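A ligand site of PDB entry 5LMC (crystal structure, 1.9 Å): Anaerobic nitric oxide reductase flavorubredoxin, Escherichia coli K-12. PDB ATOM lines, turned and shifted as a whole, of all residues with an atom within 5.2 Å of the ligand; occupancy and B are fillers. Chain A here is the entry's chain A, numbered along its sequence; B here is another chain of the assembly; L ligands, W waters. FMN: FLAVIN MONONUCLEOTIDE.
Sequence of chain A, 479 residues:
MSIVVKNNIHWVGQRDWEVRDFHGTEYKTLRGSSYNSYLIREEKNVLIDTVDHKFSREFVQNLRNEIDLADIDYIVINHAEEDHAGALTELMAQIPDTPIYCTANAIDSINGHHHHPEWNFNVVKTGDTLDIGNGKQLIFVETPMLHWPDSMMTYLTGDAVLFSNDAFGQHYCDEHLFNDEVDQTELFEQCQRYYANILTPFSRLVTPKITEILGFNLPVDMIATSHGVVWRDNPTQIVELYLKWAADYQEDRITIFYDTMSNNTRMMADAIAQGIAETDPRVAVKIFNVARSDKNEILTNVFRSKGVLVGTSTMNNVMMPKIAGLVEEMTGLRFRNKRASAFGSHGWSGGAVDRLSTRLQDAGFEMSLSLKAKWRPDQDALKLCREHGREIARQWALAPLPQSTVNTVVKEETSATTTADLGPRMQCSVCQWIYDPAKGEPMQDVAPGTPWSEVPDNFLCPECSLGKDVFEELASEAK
The backbone carbonyl oxygen (O) of Thr 314 lies within hydrogen-bond range of an oxygen (O2') of the ligand (2.9 Å).
An oxygen (O2P) of the ligand is in hydrogen-bond range of the side-chain hydroxyl (OG) of Ser 313 (2.7 Å).
The side-chain hydroxyl of Ser 345 sits at hydrogen-bond distance from an oxygen (O4') of the ligand (2.7 Å).
The backbone NH (N) of Ser 349 sits at hydrogen-bond distance from an oxygen (O2) of the ligand.
The side-chain amide nitrogen of Asn 317 lies within hydrogen-bond range of an oxygen (O4) of the ligand (3.5 Å).
The backbone NH (N) of Ser 262 sits at hydrogen-bond distance from an oxygen (O3P) of the ligand.
An oxygen (O4) of the ligand is in hydrogen-bond range of the backbone NH (N) of Asn 317 (2.7 Å).
N of Met 261 sits at hydrogen-bond distance from O2P of the ligand, at 2.7 Å.
O2 of the ligand sits at hydrogen-bond distance from N of Gly 350 (2.8 Å).
The backbone NH (N) of Thr 265 sits at hydrogen-bond distance from an oxygen (O1P) of the ligand (2.7 Å).
N of Asn 263 lies within hydrogen-bond range of O3P of the ligand, 3.1 Å away.
The side-chain hydroxyl of Thr 260 lies within hydrogen-bond range of an oxygen (O1P) of the ligand, 2.7 Å away.
O1P of the ligand lies within hydrogen-bond range of OG1 of Thr 265, at 2.7 Å.
N1 of the ligand lies within hydrogen-bond range of N of Gly 347, 3.2 Å away.
An oxygen (O3P) of the ligand sits at hydrogen-bond distance from the side-chain hydroxyl (OG) of Ser 262, at 2.6 Å.
N of Asn 316 is in hydrogen-bond range of N5 of the ligand (3.0 Å).
The side-chain amide nitrogen (ND2) of Asn 264 is in hydrogen-bond range of an oxygen (O4') of the ligand, at 2.9 Å.
The backbone NH of Trp 348 lies within hydrogen-bond range of an oxygen (O2) of the ligand (2.8 Å).
An oxygen (O3P) of the ligand is in hydrogen-bond range of the backbone NH of Asn 264 (2.9 Å).
Met 315 touches the ligand (CA to N5, 3.7 Å).
His 346 touches the ligand (CA to O2', 3.4 Å).
Trp 375 touches the ligand (CZ3 to O3', 3.3 Å).
His 23 of chain B touches the ligand (NE2 to C8M, 3.6 Å).
Glu 81 of chain B touches the ligand (OE1 to C8M, 3.6 Å).
Trp 148 of chain B touches the ligand (NE1 to C9, 3.6 Å).
Hydrophobic or aromatic side chains that line the ligand: Met 261, His 346, Trp 348, Trp 375 and His 23 of chain B.
Of the 28 residues printed, 21 come within 4 Å of the ligand.
Along chain A the residues within 4 Å of the ligand span positions 260 to 375.
Water W2 lies within hydrogen-bond range of NE2 of His 113 of chain B (2.7 Å), O3' of the ligand (2.8 Å), OG of Ser 262 (2.9 Å) and ND2 of Asn 264 (3.0 Å).
Water W3 bridges O3' of the ligand (2.8 Å) and OG of Ser 262 (3.0 Å).
Water W4 lies within hydrogen-bond range of the side-chain hydroxyl (OG) of Ser 349 (2.6 Å), the backbone carbonyl oxygen (O) of Gly 350 (2.7 Å), a nitrogen (N3) of the ligand (2.8 Å) and the side-chain amide nitrogen (ND2) of Asn 317 (2.9 Å).
Water W5 bridges a nitrogen (N5) of the ligand (3.0 Å) and the side-chain amide oxygen of Asn 316 (3.1 Å).
The side-chain hydroxyl (OG1) of Thr 260 lies within hydrogen-bond range of the backbone NH (N) of Asn 263, 2.9 Å away.
OD1 of Asn 264 sits at hydrogen-bond distance from NE of Arg 376, 2.9 Å away.
The backbone carbonyl oxygen of Ser 345 is in hydrogen-bond range of the backbone NH of Thr 314 (3.3 Å).
N of Asn 264 is in hydrogen-bond range of OG1 of Thr 260, at 3.5 Å.
The backbone NH (N) of Thr 260 is in hydrogen-bond range of the side-chain sulfur (SD) of Met 320, at 3.5 Å.
OE2 of Glu 81 of chain B lies within hydrogen-bond range of NE2 of His 147 of chain B (3.2 Å).
The backbone carbonyl oxygen (O) of Trp 375 lies close to the side-chain amide nitrogen (ND2) of Asn 264 (3.4 Å).
O of Ser 262 is in hydrogen-bond range of NH2 of Arg 376 (3.0 Å).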
ATOM      1  N   ASP A 259      17.206  15.607 -17.822  1.00  0.00           N
ATOM      2  CA  ASP A 259      17.651  16.909 -18.279  1.00  0.00           C
ATOM      3  C   ASP A 259      17.999  17.693 -17.025  1.00  0.00           C
ATOM      4  O   ASP A 259      17.597  17.299 -15.931  1.00  0.00           O
ATOM      5  CB  ASP A 259      16.583  17.617 -19.115  1.00  0.00           C
ATOM      6  CG  ASP A 259      17.174  18.600 -20.124  1.00  0.00           C
ATOM      7  OD1 ASP A 259      18.341  19.036 -19.952  1.00  0.00           O
ATOM      8  OD2 ASP A 259      16.476  18.927 -21.110  1.00  0.00           O
ATOM      9  N   THR A 260      18.727  18.785 -17.188  1.00  0.00           N
ATOM     10  CA  THR A 260      19.260  19.520 -16.047  1.00  0.00           C
ATOM     11  C   THR A 260      19.599  20.947 -16.504  1.00  0.00           C
ATOM     12  O   THR A 260      19.992  21.172 -17.649  1.00  0.00           O
ATOM     13  CB  THR A 260      20.504  18.813 -15.472  1.00  0.00           C
ATOM     14  OG1 THR A 260      20.992  19.500 -14.304  1.00  0.00           O
ATOM     15  CG2 THR A 260      21.615  18.752 -16.523  1.00  0.00           C
ATOM     16  N   MET A 261      19.400  21.921 -15.616  1.00  0.00           N
ATOM     17  CA  MET A 261      19.632  23.325 -15.944  1.00  0.00           C
ATOM     18  C   MET A 261      20.953  23.813 -15.365  1.00  0.00           C
ATOM     19  O   MET A 261      21.594  24.692 -15.928  1.00  0.00           O
ATOM     20  CB  MET A 261      18.477  24.226 -15.414  1.00  0.00           C
ATOM     21  CG  MET A 261      17.124  24.013 -16.095  1.00  0.00           C
ATOM     22  SD  MET A 261      15.808  25.125 -15.516  1.00  0.00           S
ATOM     23  CE  MET A 261      15.472  24.437 -13.883  1.00  0.00           C
ATOM     24  N   SER A 262      21.339  23.259 -14.211  1.00  0.00           N
ATOM     25  CA  SER A 262      22.588  23.673 -13.548  1.00  0.00           C
ATOM     26  C   SER A 262      23.378  22.474 -13.016  1.00  0.00           C
ATOM     27  O   SER A 262      24.154  22.592 -12.060  1.00  0.00           O
ATOM     28  CB  SER A 262      22.300  24.657 -12.407  1.00  0.00           C
ATOM     29  OG  SER A 262      21.276  24.182 -11.537  1.00  0.00           O
ATOM     30  N   ASN A 263      23.133  21.311 -13.616  1.00  0.00           N
ATOM     31  CA  ASN A 263      23.896  20.078 -13.322  1.00  0.00           C
ATOM     32  C   ASN A 263      23.621  19.350 -12.014  1.00  0.00           C
ATOM     33  O   ASN A 263      24.307  18.384 -11.699  1.00  0.00           O
ATOM     34  CB  ASN A 263      25.394  20.296 -13.455  1.00  0.00           C
ATOM     35  CG  ASN A 263      25.925  19.776 -14.754  1.00  0.00           C
ATOM     36  OD1 ASN A 263      25.332  20.013 -15.818  1.00  0.00           O
ATOM     37  ND2 ASN A 263      27.022  19.040 -14.690  1.00  0.00           N
ATOM     38  N   ASN A 264      22.617  19.798 -11.259  1.00  0.00           N
ATOM     39  CA  ASN A 264      22.344  19.159  -9.973  1.00  0.00           C
ATOM     40  C   ASN A 264      21.765  17.759 -10.163  1.00  0.00           C
ATOM     41  O   ASN A 264      22.181  16.815  -9.486  1.00  0.00           O
ATOM     42  CB  ASN A 264      21.406  20.018  -9.125  1.00  0.00           C
ATOM     43  CG  ASN A 264      22.044  21.339  -8.727  1.00  0.00           C
ATOM     44  OD1 ASN A 264      23.261  21.413  -8.610  1.00  0.00           O
ATOM     45  ND2 ASN A 264      21.233  22.371  -8.494  1.00  0.00           N
ATOM     46  N   THR A 265      20.812  17.639 -11.083  1.00  0.00           N
ATOM     47  CA  THR A 265      20.219  16.344 -11.395  1.00  0.00           C
ATOM     48  C   THR A 265      21.241  15.428 -12.079  1.00  0.00           C
ATOM     49  O   THR A 265      21.211  14.206 -11.903  1.00  0.00           O
ATOM     50  CB  THR A 265      18.953  16.537 -12.269  1.00  0.00           C
ATOM     51  OG1 THR A 265      18.015  17.364 -11.544  1.00  0.00           O
ATOM     52  CG2 THR A 265      18.293  15.201 -12.591  1.00  0.00           C
ATOM     53  N   ARG A 266      22.179  16.019 -12.816  1.00  0.00           N
ATOM     54  CA  ARG A 266      23.289  15.239 -13.381  1.00  0.00           C
ATOM     55  C   ARG A 266      24.164  14.625 -12.284  1.00  0.00           C
ATOM     56  O   ARG A 266      24.567  13.465 -12.371  1.00  0.00           O
ATOM     57  CB  ARG A 266      24.186  16.110 -14.264  1.00  0.00           C
ATOM     58  CG  ARG A 266      25.327  15.288 -14.827  1.00  0.00           C
ATOM     59  CD  ARG A 266      26.502  16.108 -15.271  1.00  0.00           C
ATOM     60  NE  ARG A 266      27.535  15.203 -15.785  1.00  0.00           N
ATOM     61  CZ  ARG A 266      28.552  15.571 -16.543  1.00  0.00           C
ATOM     62  NH1 ARG A 266      28.712  16.847 -16.882  1.00  0.00           N
ATOM     63  NH2 ARG A 266      29.416  14.655 -16.965  1.00  0.00           N
ATOM     64  N   SER A 313      14.729  18.442 -13.075  1.00  0.00           N
ATOM     65  CA  SER A 313      14.563  19.436 -12.022  1.00  0.00           C
ATOM     66  C   SER A 313      13.168  20.028 -12.158  1.00  0.00           C
ATOM     67  O   SER A 313      12.444  19.711 -13.112  1.00  0.00           O
ATOM     68  CB  SER A 313      15.633  20.517 -12.104  1.00  0.00           C
ATOM     69  OG  SER A 313      15.787  20.983 -13.434  1.00  0.00           O
ATOM     70  N   THR A 314      12.763  20.875 -11.212  1.00  0.00           N
ATOM     71  CA  THR A 314      11.509  21.618 -11.349  1.00  0.00           C
ATOM     72  C   THR A 314      11.801  22.947 -12.029  1.00  0.00           C
ATOM     73  O   THR A 314      12.687  23.688 -11.601  1.00  0.00           O
ATOM     74  CB  THR A 314      10.811  21.885 -10.011  1.00  0.00           C
ATOM     75  OG1 THR A 314      10.485  20.627  -9.398  1.00  0.00           O
ATOM     76  CG2 THR A 314       9.507  22.694 -10.240  1.00  0.00           C
ATOM     77  N   MET A 315      11.047  23.235 -13.091  1.00  0.00           N
ATOM     78  CA  MET A 315      11.206  24.476 -13.860  1.00  0.00           C
ATOM     79  C   MET A 315       9.843  25.135 -14.031  1.00  0.00           C
ATOM     80  O   MET A 315       8.975  24.602 -14.731  1.00  0.00           O
ATOM     81  CB  MET A 315      11.800  24.140 -15.227  1.00  0.00           C
ATOM     82  CG  MET A 315      11.957  25.343 -16.189  1.00  0.00           C
ATOM     83  SD  MET A 315      12.414  24.774 -17.860  1.00  0.00           S
ATOM     84  CE  MET A 315      12.419  26.318 -18.773  1.00  0.00           C
ATOM     85  N   ASN A 316       9.651  26.308 -13.419  1.00  0.00           N
ATOM     86  CA  ASN A 316       8.341  26.979 -13.434  1.00  0.00           C
ATOM     87  C   ASN A 316       7.197  26.042 -13.006  1.00  0.00           C
ATOM     88  O   ASN A 316       6.180  25.935 -13.701  1.00  0.00           O
ATOM     89  CB  ASN A 316       8.037  27.592 -14.818  1.00  0.00           C
ATOM     90  CG  ASN A 316       9.153  28.518 -15.333  1.00  0.00           C
ATOM     91  OD1 ASN A 316       9.687  29.328 -14.578  1.00  0.00           O
ATOM     92  ND2 ASN A 316       9.497  28.383 -16.605  1.00  0.00           N
ATOM     93  N   ASN A 317       7.383  25.359 -11.869  1.00  0.00           N
ATOM     94  CA  ASN A 317       6.401  24.394 -11.330  1.00  0.00           C
ATOM     95  C   ASN A 317       6.045  23.207 -12.215  1.00  0.00           C
ATOM     96  O   ASN A 317       5.110  22.469 -11.887  1.00  0.00           O
ATOM     97  CB  ASN A 317       5.122  25.088 -10.834  1.00  0.00           C
ATOM     98  CG  ASN A 317       5.412  26.364 -10.072  1.00  0.00           C
ATOM     99  OD1 ASN A 317       5.278  27.457 -10.608  1.00  0.00           O
ATOM    100  ND2 ASN A 317       5.855  26.217  -8.842  1.00  0.00           N
ATOM    101  N   MET A 320      10.996  19.579 -16.826  1.00  0.00           N
ATOM    102  CA  MET A 320      11.744  20.135 -17.951  1.00  0.00           C
ATOM    103  C   MET A 320      11.123  19.602 -19.252  1.00  0.00           C
ATOM    104  O   MET A 320      10.748  18.443 -19.334  1.00  0.00           O
ATOM    105  CB  MET A 320      13.228  19.831 -17.839  1.00  0.00           C
ATOM    106  CG  MET A 320      13.927  20.745 -16.815  1.00  0.00           C
ATOM    107  SD  MET A 320      15.704  20.552 -16.762  1.00  0.00           S
ATOM    108  CE  MET A 320      16.161  21.406 -18.279  1.00  0.00           C
ATOM    109  N   SER A 345      16.278  17.383  -8.772  1.00  0.00           N
ATOM    110  CA  SER A 345      16.520  18.445  -7.802  1.00  0.00           C
ATOM    111  C   SER A 345      15.466  19.572  -7.909  1.00  0.00           C
ATOM    112  O   SER A 345      14.758  19.702  -8.903  1.00  0.00           O
ATOM    113  CB  SER A 345      17.932  19.019  -8.012  1.00  0.00           C
ATOM    114  OG  SER A 345      18.219  20.053  -7.087  1.00  0.00           O
ATOM    115  N   HIS A 346      15.341  20.372  -6.860  1.00  0.00           N
ATOM    116  CA  HIS A 346      14.435  21.513  -6.857  1.00  0.00           C
ATOM    117  C   HIS A 346      15.030  22.596  -5.974  1.00  0.00           C
ATOM    118  O   HIS A 346      15.903  22.333  -5.144  1.00  0.00           O
ATOM    119  CB  HIS A 346      13.047  21.120  -6.321  1.00  0.00           C
ATOM    120  CG  HIS A 346      13.054  20.734  -4.881  1.00  0.00           C
ATOM    121  ND1 HIS A 346      13.499  19.507  -4.443  1.00  0.00           N
ATOM    122  CD2 HIS A 346      12.711  21.435  -3.773  1.00  0.00           C
ATOM    123  CE1 HIS A 346      13.408  19.453  -3.126  1.00  0.00           C
ATOM    124  NE2 HIS A 346      12.939  20.614  -2.689  1.00  0.00           N
ATOM    125  N   GLY A 347      14.531  23.817  -6.140  1.00  0.00           N
ATOM    126  CA  GLY A 347      15.014  24.959  -5.369  1.00  0.00           C
ATOM    127  C   GLY A 347      14.141  25.339  -4.189  1.00  0.00           C
ATOM    128  O   GLY A 347      14.630  25.797  -3.160  1.00  0.00           O
ATOM    129  N   TRP A 348      12.827  25.171  -4.321  1.00  0.00           N
ATOM    130  CA  TRP A 348      11.941  25.582  -3.236  1.00  0.00           C
ATOM    131  C   TRP A 348      10.765  24.639  -3.013  1.00  0.00           C
ATOM    132  O   TRP A 348      10.847  23.749  -2.171  1.00  0.00           O
ATOM    133  CB  TRP A 348      11.502  27.065  -3.330  1.00  0.00           C
ATOM    134  CG  TRP A 348      11.040  27.556  -4.674  1.00  0.00           C
ATOM    135  CD1 TRP A 348       9.744  27.721  -5.095  1.00  0.00           C
ATOM    136  CD2 TRP A 348      11.874  28.000  -5.767  1.00  0.00           C
ATOM    137  NE1 TRP A 348       9.725  28.216  -6.385  1.00  0.00           N
ATOM    138  CE2 TRP A 348      11.009  28.393  -6.821  1.00  0.00           C
ATOM    139  CE3 TRP A 348      13.256  28.093  -5.957  1.00  0.00           C
ATOM    140  CZ2 TRP A 348      11.491  28.867  -8.041  1.00  0.00           C
ATOM    141  CZ3 TRP A 348      13.737  28.563  -7.164  1.00  0.00           C
ATOM    142  CH2 TRP A 348      12.866  28.944  -8.200  1.00  0.00           C
ATOM    143  N   SER A 349       9.702  24.812  -3.779  1.00  0.00           N
ATOM    144  CA  SER A 349       8.523  23.975  -3.603  1.00  0.00           C
ATOM    145  C   SER A 349       8.507  22.699  -4.470  1.00  0.00           C
ATOM    146  O   SER A 349       7.744  21.791  -4.208  1.00  0.00           O
ATOM    147  CB  SER A 349       7.240  24.797  -3.811  1.00  0.00           C
ATOM    148  OG  SER A 349       7.299  25.526  -5.024  1.00  0.00           O
ATOM    149  N   GLY A 350       9.361  22.647  -5.486  1.00  0.00           N
ATOM    150  CA  GLY A 350       9.489  21.461  -6.330  1.00  0.00           C
ATOM    151  C   GLY A 350       8.171  20.987  -6.950  1.00  0.00           C
ATOM    152  O   GLY A 350       7.287  21.794  -7.218  1.00  0.00           O
ATOM    153  N   LYS A 374      17.569  18.893  -2.765  1.00  0.00           N
ATOM    154  CA  LYS A 374      17.377  20.335  -2.869  1.00  0.00           C
ATOM    155  C   LYS A 374      18.670  21.024  -3.307  1.00  0.00           C
ATOM    156  O   LYS A 374      19.757  20.749  -2.771  1.00  0.00           O
ATOM    157  CB  LYS A 374      16.886  20.908  -1.535  1.00  0.00           C
ATOM    158  CG  LYS A 374      16.575  22.397  -1.554  1.00  0.00           C
ATOM    159  CD  LYS A 374      16.100  22.849  -0.179  1.00  0.00           C
ATOM    160  CE  LYS A 374      15.467  24.226  -0.215  1.00  0.00           C
ATOM    161  NZ  LYS A 374      15.216  24.705   1.173  1.00  0.00           N
ATOM    162  N   TRP A 375      18.559  21.906  -4.297  1.00  0.00           N
ATOM    163  CA  TRP A 375      19.719  22.589  -4.879  1.00  0.00           C
ATOM    164  C   TRP A 375      20.811  21.567  -5.236  1.00  0.00           C
ATOM    165  O   TRP A 375      20.515  20.503  -5.768  1.00  0.00           O
ATOM    166  CB  TRP A 375      20.274  23.656  -3.921  1.00  0.00           C
ATOM    167  CG  TRP A 375      19.309  24.773  -3.555  1.00  0.00           C
ATOM    168  CD1 TRP A 375      18.868  25.096  -2.290  1.00  0.00           C
ATOM    169  CD2 TRP A 375      18.683  25.706  -4.447  1.00  0.00           C
ATOM    170  NE1 TRP A 375      18.017  26.169  -2.352  1.00  0.00           N
ATOM    171  CE2 TRP A 375      17.883  26.567  -3.659  1.00  0.00           C
ATOM    172  CE3 TRP A 375      18.723  25.911  -5.827  1.00  0.00           C
ATOM    173  CZ2 TRP A 375      17.128  27.599  -4.210  1.00  0.00           C
ATOM    174  CZ3 TRP A 375      17.979  26.951  -6.375  1.00  0.00           C
ATOM    175  CH2 TRP A 375      17.198  27.767  -5.564  1.00  0.00           C
ATOM    176  N   ARG A 376      22.058  21.905  -4.959  1.00  0.00           N
ATOM    177  CA  ARG A 376      23.182  21.058  -5.352  1.00  0.00           C
ATOM    178  C   ARG A 376      23.580  20.092  -4.242  1.00  0.00           C
ATOM    179  O   ARG A 376      23.903  20.515  -3.129  1.00  0.00           O
ATOM    180  CB  ARG A 376      24.386  21.931  -5.754  1.00  0.00           C
ATOM    181  CG  ARG A 376      25.637  21.135  -6.175  1.00  0.00           C
ATOM    182  CD  ARG A 376      26.578  22.047  -6.974  1.00  0.00           C
ATOM    183  NE  ARG A 376      25.869  22.569  -8.140  1.00  0.00           N
ATOM    184  CZ  ARG A 376      26.125  23.719  -8.734  1.00  0.00           C
ATOM    185  NH1 ARG A 376      27.101  24.508  -8.300  1.00  0.00           N
ATOM    186  NH2 ARG A 376      25.394  24.090  -9.781  1.00  0.00           N
ATOM    187  N   HIS B  23      20.528  27.631 -18.794  1.00  0.00           N
ATOM    188  CA  HIS B  23      19.535  26.701 -18.222  1.00  0.00           C
ATOM    189  C   HIS B  23      19.502  25.389 -18.975  1.00  0.00           C
ATOM    190  O   HIS B  23      18.458  24.976 -19.500  1.00  0.00           O
ATOM    191  CB  HIS B  23      18.141  27.355 -18.194  1.00  0.00           C
ATOM    192  CG  HIS B  23      18.079  28.577 -17.326  1.00  0.00           C
ATOM    193  ND1 HIS B  23      17.077  29.518 -17.434  1.00  0.00           N
ATOM    194  CD2 HIS B  23      18.885  29.008 -16.328  1.00  0.00           C
ATOM    195  CE1 HIS B  23      17.280  30.480 -16.560  1.00  0.00           C
ATOM    196  NE2 HIS B  23      18.362  30.180 -15.861  1.00  0.00           N
ATOM    197  N   GLU B  81      21.848  32.508  -8.105  1.00  0.00           N
ATOM    198  CA  GLU B  81      21.986  31.629  -9.262  1.00  0.00           C
ATOM    199  C   GLU B  81      23.468  31.612  -9.702  1.00  0.00           C
ATOM    200  O   GLU B  81      24.181  32.591  -9.486  1.00  0.00           O
ATOM    201  CB  GLU B  81      21.064  32.090 -10.393  1.00  0.00           C
ATOM    202  CG  GLU B  81      20.935  31.062 -11.510  1.00  0.00           C
ATOM    203  CD  GLU B  81      19.726  31.292 -12.390  1.00  0.00           C
ATOM    204  OE1 GLU B  81      19.483  30.434 -13.275  1.00  0.00           O
ATOM    205  OE2 GLU B  81      19.046  32.333 -12.215  1.00  0.00           O
ATOM    206  N   HIS B 113      24.164  26.000  -3.006  1.00  0.00           N
ATOM    207  CA  HIS B 113      25.122  25.844  -4.098  1.00  0.00           C
ATOM    208  C   HIS B 113      26.565  25.682  -3.624  1.00  0.00           C
ATOM    209  O   HIS B 113      27.328  24.921  -4.222  1.00  0.00           O
ATOM    210  CB  HIS B 113      25.041  27.043  -5.059  1.00  0.00           C
ATOM    211  CG  HIS B 113      23.772  27.100  -5.852  1.00  0.00           C
ATOM    212  ND1 HIS B 113      22.586  27.603  -5.356  1.00  0.00           N
ATOM    213  CD2 HIS B 113      23.516  26.732  -7.137  1.00  0.00           C
ATOM    214  CE1 HIS B 113      21.654  27.533  -6.288  1.00  0.00           C
ATOM    215  NE2 HIS B 113      22.194  27.011  -7.377  1.00  0.00           N
ATOM    216  N   HIS B 147      13.603  36.735 -10.066  1.00  0.00           N
ATOM    217  CA  HIS B 147      12.738  35.630 -10.483  1.00  0.00           C
ATOM    218  C   HIS B 147      12.895  34.394  -9.583  1.00  0.00           C
ATOM    219  O   HIS B 147      12.295  33.352  -9.853  1.00  0.00           O
ATOM    220  CB  HIS B 147      13.028  35.261 -11.943  1.00  0.00           C
ATOM    221  CG  HIS B 147      14.397  34.689 -12.177  1.00  0.00           C
ATOM    222  ND1 HIS B 147      14.613  33.340 -12.406  1.00  0.00           N
ATOM    223  CD2 HIS B 147      15.625  35.268 -12.170  1.00  0.00           C
ATOM    224  CE1 HIS B 147      15.912  33.128 -12.548  1.00  0.00           C
ATOM    225  NE2 HIS B 147      16.545  34.281 -12.419  1.00  0.00           N
ATOM    226  N   TRP B 148      13.687  34.506  -8.516  1.00  0.00           N
ATOM    227  CA  TRP B 148      13.854  33.407  -7.547  1.00  0.00           C
ATOM    228  C   TRP B 148      13.413  33.874  -6.172  1.00  0.00           C
ATOM    229  O   TRP B 148      13.339  35.068  -5.922  1.00  0.00           O
ATOM    230  CB  TRP B 148      15.326  32.952  -7.465  1.00  0.00           C
ATOM    231  CG  TRP B 148      15.763  31.867  -8.423  1.00  0.00           C
ATOM    232  CD1 TRP B 148      15.100  31.419  -9.540  1.00  0.00           C
ATOM    233  CD2 TRP B 148      16.970  31.097  -8.336  1.00  0.00           C
ATOM    234  NE1 TRP B 148      15.827  30.415 -10.156  1.00  0.00           N
ATOM    235  CE2 TRP B 148      16.971  30.202  -9.431  1.00  0.00           C
ATOM    236  CE3 TRP B 148      18.049  31.088  -7.438  1.00  0.00           C
ATOM    237  CZ2 TRP B 148      18.012  29.285  -9.650  1.00  0.00           C
ATOM    238  CZ3 TRP B 148      19.096  30.177  -7.662  1.00  0.00           C
ATOM    239  CH2 TRP B 148      19.061  29.294  -8.762  1.00  0.00           C
HETATM  240  N1  FMN L   1      12.534  25.327  -8.131  1.00  0.00           N
HETATM  241  C2  FMN L   1      11.312  25.018  -7.573  1.00  0.00           C
HETATM  242  O2  FMN L   1      11.254  24.422  -6.486  1.00  0.00           O
HETATM  243  N3  FMN L   1      10.155  25.379  -8.240  1.00  0.00           N
HETATM  244  C4  FMN L   1      10.184  26.042  -9.455  1.00  0.00           C
HETATM  245  O4  FMN L   1       9.114  26.351 -10.010  1.00  0.00           O
HETATM  246  C4A FMN L   1      11.419  26.341 -10.032  1.00  0.00           C
HETATM  247  N5  FMN L   1      11.516  27.008 -11.242  1.00  0.00           N
HETATM  248  C5A FMN L   1      12.762  27.292 -11.785  1.00  0.00           C
HETATM  249  C6  FMN L   1      12.878  27.951 -13.005  1.00  0.00           C
HETATM  250  C7  FMN L   1      14.141  28.222 -13.544  1.00  0.00           C
HETATM  251  C7M FMN L   1      14.267  28.933 -14.865  1.00  0.00           C
HETATM  252  C8  FMN L   1      15.291  27.863 -12.861  1.00  0.00           C
HETATM  253  C8M FMN L   1      16.648  28.174 -13.441  1.00  0.00           C
HETATM  254  C9  FMN L   1      15.186  27.199 -11.635  1.00  0.00           C
HETATM  255  C9A FMN L   1      13.924  26.914 -11.093  1.00  0.00           C
HETATM  256  N10 FMN L   1      13.814  26.266  -9.892  1.00  0.00           N
HETATM  257  C10 FMN L   1      12.581  25.977  -9.342  1.00  0.00           C
HETATM  258  C1' FMN L   1      15.037  25.863  -9.123  1.00  0.00           C
HETATM  259  C2' FMN L   1      15.691  24.602  -9.637  1.00  0.00           C
HETATM  260  O2' FMN L   1      14.771  23.529  -9.552  1.00  0.00           O
HETATM  261  C3' FMN L   1      16.946  24.343  -8.802  1.00  0.00           C
HETATM  262  O3' FMN L   1      17.942  25.249  -9.240  1.00  0.00           O
HETATM  263  C4' FMN L   1      17.439  22.908  -9.025  1.00  0.00           C
HETATM  264  O4' FMN L   1      18.412  22.555  -8.057  1.00  0.00           O
HETATM  265  C5' FMN L   1      18.025  22.753 -10.427  1.00  0.00           C
HETATM  266  O5' FMN L   1      18.370  21.400 -10.674  1.00  0.00           O
HETATM  267  P   FMN L   1      19.182  21.085 -12.022  1.00  0.00           P
HETATM  268  O1P FMN L   1      19.344  19.602 -12.188  1.00  0.00           O
HETATM  269  O2P FMN L   1      18.397  21.695 -13.161  1.00  0.00           O
HETATM  270  O3P FMN L   1      20.566  21.736 -11.982  1.00  0.00           O
HETATM  271  O   HOH W   1      12.824  31.572 -13.436  1.00  0.00           O
HETATM  272  O   HOH W   2      20.724  25.317  -8.949  1.00  0.00           O
HETATM  273  O   HOH W   3      18.809  25.874 -11.834  1.00  0.00           O
HETATM  274  O   HOH W   4       7.642  24.488  -7.364  1.00  0.00           O
HETATM  275  O   HOH W   5       9.769  29.413 -11.504  1.00  0.00           O
